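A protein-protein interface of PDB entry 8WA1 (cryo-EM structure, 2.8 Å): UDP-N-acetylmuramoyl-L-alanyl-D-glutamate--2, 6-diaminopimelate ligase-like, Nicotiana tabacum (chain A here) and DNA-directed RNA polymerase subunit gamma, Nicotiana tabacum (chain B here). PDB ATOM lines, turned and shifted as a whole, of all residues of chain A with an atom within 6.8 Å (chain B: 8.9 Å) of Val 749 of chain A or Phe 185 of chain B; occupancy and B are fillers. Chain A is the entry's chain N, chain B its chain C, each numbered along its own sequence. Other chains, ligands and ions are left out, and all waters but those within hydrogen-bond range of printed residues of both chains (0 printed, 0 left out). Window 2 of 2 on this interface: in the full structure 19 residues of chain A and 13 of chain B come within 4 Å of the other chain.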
ATOM      1  N   ALA A 587      11.787  -4.153  25.039  1.00  0.00           N
ATOM      2  CA  ALA A 587      11.369  -2.787  25.316  1.00  0.00           C
ATOM      3  C   ALA A 587      11.465  -2.545  26.813  1.00  0.00           C
ATOM      4  O   ALA A 587      11.784  -3.455  27.583  1.00  0.00           O
ATOM      5  CB  ALA A 587       9.942  -2.517  24.823  1.00  0.00           C
ATOM      6  N   PHE A 588      11.188  -1.307  27.211  1.00  0.00           N
ATOM      7  CA  PHE A 588      11.207  -0.936  28.615  1.00  0.00           C
ATOM      8  C   PHE A 588      10.054  -1.602  29.364  1.00  0.00           C
ATOM      9  O   PHE A 588       9.132  -2.167  28.769  1.00  0.00           O
ATOM     10  CB  PHE A 588      11.135   0.583  28.762  1.00  0.00           C
ATOM     11  CG  PHE A 588      10.553   1.278  27.564  1.00  0.00           C
ATOM     12  CD1 PHE A 588       9.182   1.365  27.395  1.00  0.00           C
ATOM     13  CD2 PHE A 588      11.378   1.839  26.602  1.00  0.00           C
ATOM     14  CE1 PHE A 588       8.646   2.000  26.293  1.00  0.00           C
ATOM     15  CE2 PHE A 588      10.845   2.476  25.497  1.00  0.00           C
ATOM     16  CZ  PHE A 588       9.478   2.556  25.343  1.00  0.00           C
ATOM     17  N   ARG A 700      -7.059   5.174  25.224  1.00  0.00           N
ATOM     18  CA  ARG A 700      -6.204   4.490  24.256  1.00  0.00           C
ATOM     19  C   ARG A 700      -4.995   5.340  23.881  1.00  0.00           C
ATOM     20  O   ARG A 700      -3.855   4.859  23.917  1.00  0.00           O
ATOM     21  CB  ARG A 700      -7.014   4.124  23.011  1.00  0.00           C
ATOM     22  CG  ARG A 700      -6.175   3.797  21.783  1.00  0.00           C
ATOM     23  CD  ARG A 700      -5.284   2.581  21.998  1.00  0.00           C
ATOM     24  NE  ARG A 700      -4.384   2.368  20.869  1.00  0.00           N
ATOM     25  CZ  ARG A 700      -3.364   1.516  20.876  1.00  0.00           C
ATOM     26  NH1 ARG A 700      -3.108   0.796  21.958  1.00  0.00           N
ATOM     27  NH2 ARG A 700      -2.597   1.388  19.802  1.00  0.00           N
ATOM     28  N   VAL A 701      -5.223   6.602  23.512  1.00  0.00           N
ATOM     29  CA  VAL A 701      -4.113   7.462  23.111  1.00  0.00           C
ATOM     30  C   VAL A 701      -3.212   7.758  24.303  1.00  0.00           C
ATOM     31  O   VAL A 701      -1.994   7.915  24.155  1.00  0.00           O
ATOM     32  CB  VAL A 701      -4.641   8.751  22.452  1.00  0.00           C
ATOM     33  CG1 VAL A 701      -5.545   8.407  21.278  1.00  0.00           C
ATOM     34  CG2 VAL A 701      -5.378   9.612  23.461  1.00  0.00           C
ATOM     35  N   VAL A 703      -2.583   5.613  26.843  1.00  0.00           N
ATOM     36  CA  VAL A 703      -1.761   4.420  27.030  1.00  0.00           C
ATOM     37  C   VAL A 703      -0.702   4.329  25.940  1.00  0.00           C
ATOM     38  O   VAL A 703       0.442   3.934  26.198  1.00  0.00           O
ATOM     39  CB  VAL A 703      -2.645   3.160  27.069  1.00  0.00           C
ATOM     40  N   ARG A 704      -1.056   4.706  24.710  1.00  0.00           N
ATOM     41  CA  ARG A 704      -0.088   4.684  23.619  1.00  0.00           C
ATOM     42  C   ARG A 704       1.030   5.699  23.810  1.00  0.00           C
ATOM     43  O   ARG A 704       2.193   5.373  23.552  1.00  0.00           O
ATOM     44  CB  ARG A 704      -0.792   4.939  22.286  1.00  0.00           C
ATOM     45  N   CYS A 705       0.711   6.910  24.275  1.00  0.00           N
ATOM     46  CA  CYS A 705       1.749   7.899  24.537  1.00  0.00           C
ATOM     47  C   CYS A 705       2.609   7.493  25.727  1.00  0.00           C
ATOM     48  O   CYS A 705       3.814   7.768  25.749  1.00  0.00           O
ATOM     49  CB  CYS A 705       1.118   9.271  24.770  1.00  0.00           C
ATOM     50  N   VAL A 707       3.273   4.338  26.600  1.00  0.00           N
ATOM     51  CA  VAL A 707       4.108   3.237  26.138  1.00  0.00           C
ATOM     52  C   VAL A 707       5.107   3.667  25.078  1.00  0.00           C
ATOM     53  O   VAL A 707       6.086   2.952  24.838  1.00  0.00           O
ATOM     54  CB  VAL A 707       3.235   2.088  25.594  1.00  0.00           C
ATOM     55  N   ALA A 708       4.888   4.814  24.437  1.00  0.00           N
ATOM     56  CA  ALA A 708       5.841   5.369  23.489  1.00  0.00           C
ATOM     57  C   ALA A 708       6.862   6.284  24.148  1.00  0.00           C
ATOM     58  O   ALA A 708       7.932   6.512  23.572  1.00  0.00           O
ATOM     59  CB  ALA A 708       5.106   6.136  22.381  1.00  0.00           C
ATOM     60  N   MET A 709       6.560   6.811  25.332  1.00  0.00           N
ATOM     61  CA  MET A 709       7.494   7.643  26.088  1.00  0.00           C
ATOM     62  C   MET A 709       8.205   6.752  27.098  1.00  0.00           C
ATOM     63  O   MET A 709       7.681   6.479  28.179  1.00  0.00           O
ATOM     64  CB  MET A 709       6.762   8.791  26.771  1.00  0.00           C
ATOM     65  N   GLU A 741      -3.066  -4.060  23.357  1.00  0.00           N
ATOM     66  CA  GLU A 741      -2.987  -2.682  22.886  1.00  0.00           C
ATOM     67  C   GLU A 741      -1.669  -2.036  23.299  1.00  0.00           C
ATOM     68  O   GLU A 741      -1.063  -1.288  22.524  1.00  0.00           O
ATOM     69  CB  GLU A 741      -4.173  -1.881  23.421  1.00  0.00           C
ATOM     70  N   GLU A 744       1.148  -3.620  21.176  1.00  0.00           N
ATOM     71  CA  GLU A 744       1.173  -3.053  19.831  1.00  0.00           C
ATOM     72  C   GLU A 744       1.885  -1.706  19.817  1.00  0.00           C
ATOM     73  O   GLU A 744       2.576  -1.371  18.847  1.00  0.00           O
ATOM     74  CB  GLU A 744      -0.255  -2.917  19.298  1.00  0.00           C
ATOM     75  CG  GLU A 744      -0.358  -2.295  17.912  1.00  0.00           C
ATOM     76  CD  GLU A 744       0.185  -3.197  16.818  1.00  0.00           C
ATOM     77  OE1 GLU A 744       0.226  -4.428  17.026  1.00  0.00           O
ATOM     78  OE2 GLU A 744       0.570  -2.674  15.751  1.00  0.00           O
ATOM     79  N   ALA A 745       1.737  -0.925  20.890  1.00  0.00           N
ATOM     80  CA  ALA A 745       2.428   0.358  20.974  1.00  0.00           C
ATOM     81  C   ALA A 745       3.939   0.167  21.032  1.00  0.00           C
ATOM     82  O   ALA A 745       4.688   0.866  20.342  1.00  0.00           O
ATOM     83  CB  ALA A 745       1.939   1.141  22.192  1.00  0.00           C
ATOM     84  N   LEU A 746       4.405  -0.773  21.857  1.00  0.00           N
ATOM     85  CA  LEU A 746       5.834  -1.062  21.913  1.00  0.00           C
ATOM     86  C   LEU A 746       6.337  -1.609  20.584  1.00  0.00           C
ATOM     87  O   LEU A 746       7.490  -1.376  20.203  1.00  0.00           O
ATOM     88  CB  LEU A 746       6.127  -2.047  23.045  1.00  0.00           C
ATOM     89  N   GLN A 747       5.489  -2.350  19.868  1.00  0.00           N
ATOM     90  CA  GLN A 747       5.896  -2.893  18.576  1.00  0.00           C
ATOM     91  C   GLN A 747       6.022  -1.797  17.524  1.00  0.00           C
ATOM     92  O   GLN A 747       6.961  -1.808  16.717  1.00  0.00           O
ATOM     93  CB  GLN A 747       4.901  -3.962  18.122  1.00  0.00           C
ATOM     94  N   TYR A 748       5.096  -0.841  17.519  1.00  0.00           N
ATOM     95  CA  TYR A 748       5.019   0.166  16.466  1.00  0.00           C
ATOM     96  C   TYR A 748       5.671   1.495  16.836  1.00  0.00           C
ATOM     97  O   TYR A 748       5.630   2.429  16.030  1.00  0.00           O
ATOM     98  CB  TYR A 748       3.555   0.408  16.078  1.00  0.00           C
ATOM     99  N   VAL A 749       6.261   1.610  18.029  1.00  0.00           N
ATOM    100  CA  VAL A 749       6.933   2.853  18.404  1.00  0.00           C
ATOM    101  C   VAL A 749       8.138   3.110  17.504  1.00  0.00           C
ATOM    102  O   VAL A 749       8.592   4.254  17.362  1.00  0.00           O
ATOM    103  CB  VAL A 749       7.328   2.812  19.893  1.00  0.00           C
ATOM    104  CG1 VAL A 749       8.365   1.727  20.141  1.00  0.00           C
ATOM    105  CG2 VAL A 749       7.838   4.171  20.365  1.00  0.00           C
ATOM    106  N   ASP A 750       8.673   2.056  16.881  1.00  0.00           N
ATOM    107  CA  ASP A 750       9.813   2.218  15.986  1.00  0.00           C
ATOM    108  C   ASP A 750       9.480   3.087  14.780  1.00  0.00           C
ATOM    109  O   ASP A 750      10.340   3.847  14.323  1.00  0.00           O
ATOM    110  CB  ASP A 750      10.314   0.851  15.520  1.00  0.00           C
ATOM    111  N   GLU A 751       8.250   3.007  14.267  1.00  0.00           N
ATOM    112  CA  GLU A 751       7.868   3.843  13.133  1.00  0.00           C
ATOM    113  C   GLU A 751       7.859   5.317  13.516  1.00  0.00           C
ATOM    114  O   GLU A 751       8.366   6.165  12.772  1.00  0.00           O
ATOM    115  CB  GLU A 751       6.500   3.415  12.604  1.00  0.00           C
ATOM    116  N   LEU A 752       7.286   5.643  14.678  1.00  0.00           N
ATOM    117  CA  LEU A 752       7.273   7.029  15.133  1.00  0.00           C
ATOM    118  C   LEU A 752       8.682   7.519  15.443  1.00  0.00           C
ATOM    119  O   LEU A 752       8.998   8.697  15.235  1.00  0.00           O
ATOM    120  CB  LEU A 752       6.371   7.175  16.357  1.00  0.00           C
ATOM    121  CG  LEU A 752       4.883   6.893  16.147  1.00  0.00           C
ATOM    122  CD1 LEU A 752       4.106   7.214  17.412  1.00  0.00           C
ATOM    123  CD2 LEU A 752       4.345   7.686  14.967  1.00  0.00           C
ATOM    124  N   HIS A 753       9.541   6.632  15.951  1.00  0.00           N
ATOM    125  CA  HIS A 753      10.920   7.021  16.231  1.00  0.00           C
ATOM    126  C   HIS A 753      11.684   7.307  14.945  1.00  0.00           C
ATOM    127  O   HIS A 753      12.443   8.280  14.866  1.00  0.00           O
ATOM    128  CB  HIS A 753      11.619   5.930  17.042  1.00  0.00           C
ATOM    129  N   GLN A 754      11.498   6.467  13.924  1.00  0.00           N
ATOM    130  CA  GLN A 754      12.183   6.680  12.653  1.00  0.00           C
ATOM    131  C   GLN A 754      11.646   7.912  11.936  1.00  0.00           C
ATOM    132  O   GLN A 754      12.403   8.633  11.274  1.00  0.00           O
ATOM    133  CB  GLN A 754      12.045   5.441  11.769  1.00  0.00           C
ATOM    134  N   THR A 759       8.539  11.941  21.802  1.00  0.00           N
ATOM    135  CA  THR A 759       7.601  11.570  22.852  1.00  0.00           C
ATOM    136  C   THR A 759       8.114  11.917  24.246  1.00  0.00           C
ATOM    137  O   THR A 759       7.517  11.494  25.240  1.00  0.00           O
ATOM    138  CB  THR A 759       7.283  10.074  22.760  1.00  0.00           C
ATOM    139  OG1 THR A 759       7.338   9.660  21.390  1.00  0.00           O
ATOM    140  CG2 THR A 759       5.888   9.783  23.298  1.00  0.00           C
ATOM    141  N   TRP A 764       4.056  16.853  21.438  1.00  0.00           N
ATOM    142  CA  TRP A 764       4.966  16.134  20.556  1.00  0.00           C
ATOM    143  C   TRP A 764       5.486  17.080  19.481  1.00  0.00           C
ATOM    144  O   TRP A 764       4.700  17.754  18.808  1.00  0.00           O
ATOM    145  CB  TRP A 764       4.272  14.934  19.914  1.00  0.00           C
ATOM    146  CG  TRP A 764       3.971  13.814  20.862  1.00  0.00           C
ATOM    147  CD1 TRP A 764       4.165  13.805  22.211  1.00  0.00           C
ATOM    148  CD2 TRP A 764       3.428  12.530  20.527  1.00  0.00           C
ATOM    149  NE1 TRP A 764       3.773  12.600  22.739  1.00  0.00           N
ATOM    150  CE2 TRP A 764       3.317  11.799  21.726  1.00  0.00           C
ATOM    151  CE3 TRP A 764       3.024  11.931  19.331  1.00  0.00           C
ATOM    152  CZ2 TRP A 764       2.818  10.500  21.763  1.00  0.00           C
ATOM    153  CZ3 TRP A 764       2.531  10.641  19.370  1.00  0.00           C
ATOM    154  CH2 TRP A 764       2.433   9.939  20.578  1.00  0.00           C
ATOM    155  N   LYS B 179       1.544  11.353   8.926  1.00  0.00           N
ATOM    156  CA  LYS B 179       0.284  10.950   9.529  1.00  0.00           C
ATOM    157  C   LYS B 179      -0.037   9.473   9.355  1.00  0.00           C
ATOM    158  O   LYS B 179      -0.879   8.954  10.097  1.00  0.00           O
ATOM    159  CB  LYS B 179      -0.877  11.781   8.958  1.00  0.00           C
ATOM    160  CG  LYS B 179      -0.678  13.284   9.061  1.00  0.00           C
ATOM    161  CD  LYS B 179      -1.863  13.962   9.728  1.00  0.00           C
ATOM    162  CE  LYS B 179      -2.019  13.507  11.172  1.00  0.00           C
ATOM    163  NZ  LYS B 179      -3.148  14.194  11.859  1.00  0.00           N
ATOM    164  N   TYR B 180       0.594   8.781   8.400  1.00  0.00           N
ATOM    165  CA  TYR B 180       0.337   7.353   8.241  1.00  0.00           C
ATOM    166  C   TYR B 180       0.936   6.557   9.394  1.00  0.00           C
ATOM    167  O   TYR B 180       0.305   5.630   9.913  1.00  0.00           O
ATOM    168  CB  TYR B 180       0.886   6.862   6.901  1.00  0.00           C
ATOM    169  N   SER B 181       2.157   6.907   9.808  1.00  0.00           N
ATOM    170  CA  SER B 181       2.749   6.268  10.978  1.00  0.00           C
ATOM    171  C   SER B 181       1.959   6.595  12.239  1.00  0.00           C
ATOM    172  O   SER B 181       1.849   5.760  13.144  1.00  0.00           O
ATOM    173  CB  SER B 181       4.208   6.698  11.130  1.00  0.00           C
ATOM    174  N   ILE B 182       1.410   7.811  12.318  1.00  0.00           N
ATOM    175  CA  ILE B 182       0.577   8.171  13.467  1.00  0.00           C
ATOM    176  C   ILE B 182      -0.731   7.397  13.462  1.00  0.00           C
ATOM    177  O   ILE B 182      -1.167   6.951  14.534  1.00  0.00           O
ATOM    178  CB  ILE B 182       0.376   9.692  13.519  1.00  0.00           C
ATOM    179  N   PRO B 183      -1.407   7.194  12.328  1.00  0.00           N
ATOM    180  CA  PRO B 183      -2.686   6.467  12.373  1.00  0.00           C
ATOM    181  C   PRO B 183      -2.524   4.985  12.654  1.00  0.00           C
ATOM    182  O   PRO B 183      -3.328   4.407  13.396  1.00  0.00           O
ATOM    183  CB  PRO B 183      -3.278   6.722  10.979  1.00  0.00           C
ATOM    184  N   LEU B 184      -1.505   4.349  12.072  1.00  0.00           N
ATOM    185  CA  LEU B 184      -1.269   2.933  12.332  1.00  0.00           C
ATOM    186  C   LEU B 184      -0.906   2.700  13.794  1.00  0.00           C
ATOM    187  O   LEU B 184      -1.389   1.751  14.424  1.00  0.00           O
ATOM    188  CB  LEU B 184      -0.169   2.406  11.409  1.00  0.00           C
ATOM    189  N   PHE B 185      -0.053   3.562  14.346  1.00  0.00           N
ATOM    190  CA  PHE B 185       0.369   3.428  15.744  1.00  0.00           C
ATOM    191  C   PHE B 185      -0.826   3.377  16.667  1.00  0.00           C
ATOM    192  O   PHE B 185      -0.997   2.420  17.423  1.00  0.00           O
ATOM    193  CB  PHE B 185       1.260   4.603  16.138  1.00  0.00           C
ATOM    194  CG  PHE B 185       1.757   4.542  17.552  1.00  0.00           C
ATOM    195  CD1 PHE B 185       2.765   3.664  17.904  1.00  0.00           C
ATOM    196  CD2 PHE B 185       1.230   5.376  18.522  1.00  0.00           C
ATOM    197  CE1 PHE B 185       3.232   3.612  19.201  1.00  0.00           C
ATOM    198  CE2 PHE B 185       1.695   5.329  19.820  1.00  0.00           C
ATOM    199  CZ  PHE B 185       2.695   4.442  20.161  1.00  0.00           C
ATOM    200  N   PHE B 186      -1.651   4.410  16.619  1.00  0.00           N
ATOM    201  CA  PHE B 186      -2.853   4.434  17.434  1.00  0.00           C
ATOM    202  C   PHE B 186      -3.860   3.470  16.841  1.00  0.00           C
ATOM    203  O   PHE B 186      -3.749   3.086  15.686  1.00  0.00           O
ATOM    204  CB  PHE B 186      -3.441   5.844  17.487  1.00  0.00           C
ATOM    205  CG  PHE B 186      -2.552   6.848  18.163  1.00  0.00           C
ATOM    206  CD1 PHE B 186      -2.402   6.845  19.537  1.00  0.00           C
ATOM    207  CD2 PHE B 186      -1.876   7.804  17.426  1.00  0.00           C
ATOM    208  CE1 PHE B 186      -1.588   7.769  20.162  1.00  0.00           C
ATOM    209  CE2 PHE B 186      -1.058   8.729  18.043  1.00  0.00           C
ATOM    210  CZ  PHE B 186      -0.915   8.712  19.414  1.00  0.00           C
ATOM    211  N   THR B 187      -4.839   3.043  17.623  1.00  0.00           N
ATOM    212  CA  THR B 187      -5.876   2.205  17.045  1.00  0.00           C
ATOM    213  C   THR B 187      -6.553   3.067  15.992  1.00  0.00           C
ATOM    214  O   THR B 187      -6.720   4.266  16.194  1.00  0.00           O
ATOM    215  CB  THR B 187      -6.906   1.766  18.095  1.00  0.00           C
ATOM    216  N   THR B 188      -6.944   2.480  14.866  1.00  0.00           N
ATOM    217  CA  THR B 188      -7.526   3.273  13.785  1.00  0.00           C
ATOM    218  C   THR B 188      -8.799   3.957  14.247  1.00  0.00           C
ATOM    219  O   THR B 188      -9.037   5.118  13.915  1.00  0.00           O
ATOM    220  CB  THR B 188      -7.834   2.409  12.551  1.00  0.00           C
ATOM    221  N   GLY B 190      -9.373   4.794  17.280  1.00  0.00           N
ATOM    222  CA  GLY B 190      -8.888   5.837  18.170  1.00  0.00           C
ATOM    223  C   GLY B 190      -8.402   7.057  17.419  1.00  0.00           C
ATOM    224  O   GLY B 190      -8.632   8.184  17.852  1.00  0.00           O
ATOM    225  N   PHE B 191      -7.722   6.846  16.295  1.00  0.00           N
ATOM    226  CA  PHE B 191      -7.237   7.962  15.493  1.00  0.00           C
ATOM    227  C   PHE B 191      -8.414   8.764  14.985  1.00  0.00           C
ATOM    228  O   PHE B 191      -8.378   9.993  14.985  1.00  0.00           O
ATOM    229  CB  PHE B 191      -6.390   7.474  14.323  1.00  0.00           C
ATOM    230  CG  PHE B 191      -5.685   8.576  13.587  1.00  0.00           C
ATOM    231  CD1 PHE B 191      -4.518   9.123  14.092  1.00  0.00           C
ATOM    232  CD2 PHE B 191      -6.184   9.063  12.392  1.00  0.00           C
ATOM    233  CE1 PHE B 191      -3.864  10.137  13.422  1.00  0.00           C
ATOM    234  CE2 PHE B 191      -5.535  10.078  11.716  1.00  0.00           C
ATOM    235  CZ  PHE B 191      -4.372  10.615  12.231  1.00  0.00           C
ATOM    236  N   PHE B 194      -9.807  11.106  17.777  1.00  0.00           N
ATOM    237  CA  PHE B 194      -9.127  12.349  18.124  1.00  0.00           C
ATOM    238  C   PHE B 194      -8.767  13.269  16.949  1.00  0.00           C
ATOM    239  O   PHE B 194      -8.328  14.394  17.176  1.00  0.00           O
ATOM    240  CB  PHE B 194      -7.928  12.116  19.064  1.00  0.00           C
ATOM    241  CG  PHE B 194      -6.657  11.690  18.378  1.00  0.00           C
ATOM    242  CD1 PHE B 194      -6.365  10.352  18.204  1.00  0.00           C
ATOM    243  CD2 PHE B 194      -5.726  12.627  17.961  1.00  0.00           C
ATOM    244  CE1 PHE B 194      -5.192   9.955  17.596  1.00  0.00           C
ATOM    245  CE2 PHE B 194      -4.554  12.239  17.345  1.00  0.00           C
ATOM    246  CZ  PHE B 194      -4.285  10.900  17.166  1.00  0.00           C
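Of the printed residues of chain B, Arg 700 of chain A touches Phe 185 (3.0 Å), Phe 186 (3.8 Å) and Thr 187 (3.3 Å).
Ala 708 of chain A touches just one residue of chain B: Phe 185 (3.7 Å).
Of the printed residues of chain B, Ala 745 of chain A touches Phe 185 (3.3 Å).
Of the printed residues of chain B, Tyr 748 of chain A touches Phe 185.
No residue of chain B comes within 4 Å of Asp 750 of chain A.
Of the printed residues of chain B, Leu 752 of chain A touches Ser 181 (3.6 Å), Ile 182 (3.96 Å) and Phe 185 (3.6 Å).
Of the printed residues of chain A, Ser 181 of chain B touches Leu 752.
Of chain A, only Arg 700 (3.0 Å), Arg 704 (3.5 Å), Ala 708 (3.7 Å), Ala 745 (3.3 Å), Tyr 748 (3.6 Å), Val 749 (3.8 Å) and Leu 752 (3.6 Å) come within 4 Å of Phe 185 of chain B.
The nearest residue of chain B that does not touch Val 749 of chain A is Ser 181 of chain B (7.8 Å).
The nearest printed residue of chain B that does not touch Ala 745 of chain A is Phe 186 of chain B (7.2 Å).
Among the printed residues, merely in contact across the chains: Ala 745 of chain A with Phe 185 of chain B, Arg 704 of chain A with Phe 185 of chain B, Leu 752 of chain A with Phe 185 of chain B, Arg 704 of chain A with Phe 186 of chain B, Tyr 748 of chain A with Phe 185 of chain B, Leu 752 of chain A with Ser 181 of chain B, Ala 708 of chain A with Phe 185 of chain B, Val 701 of chain A with Phe 194 of chain B, Trp 764 of chain A with Phe 186 of chain B, Val 749 of chain A with Phe 185 of chain B, Arg 700 of chain A with Phe 186 of chain B, Val 701 of chain A with Phe 186 of chain B and Leu 752 of chain A with Ile 182 of chain B.
NH2 of Arg 700 of chain A lies within hydrogen-bond range of O of Phe 185 of chain B, at 3.0 Å.
The guanidinium group (NE) of Arg 700 of chain A lies close to the backbone NH (N) of Thr 187 of chain B.
Of the 13 printed residues of chain B, 6 touch a printed residue of chain A.
Of the 24 printed residues of chain A, 9 touch a printed residue of chain B.
Among the printed residues, no Asp or Glu carboxylate lies within 4 Å of a Lys or Arg side-chain nitrogen of the other chain.
NH1 of Arg 700 of chain A sits at hydrogen-bond distance from O of Glu 741 of chain A (3.0 Å).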
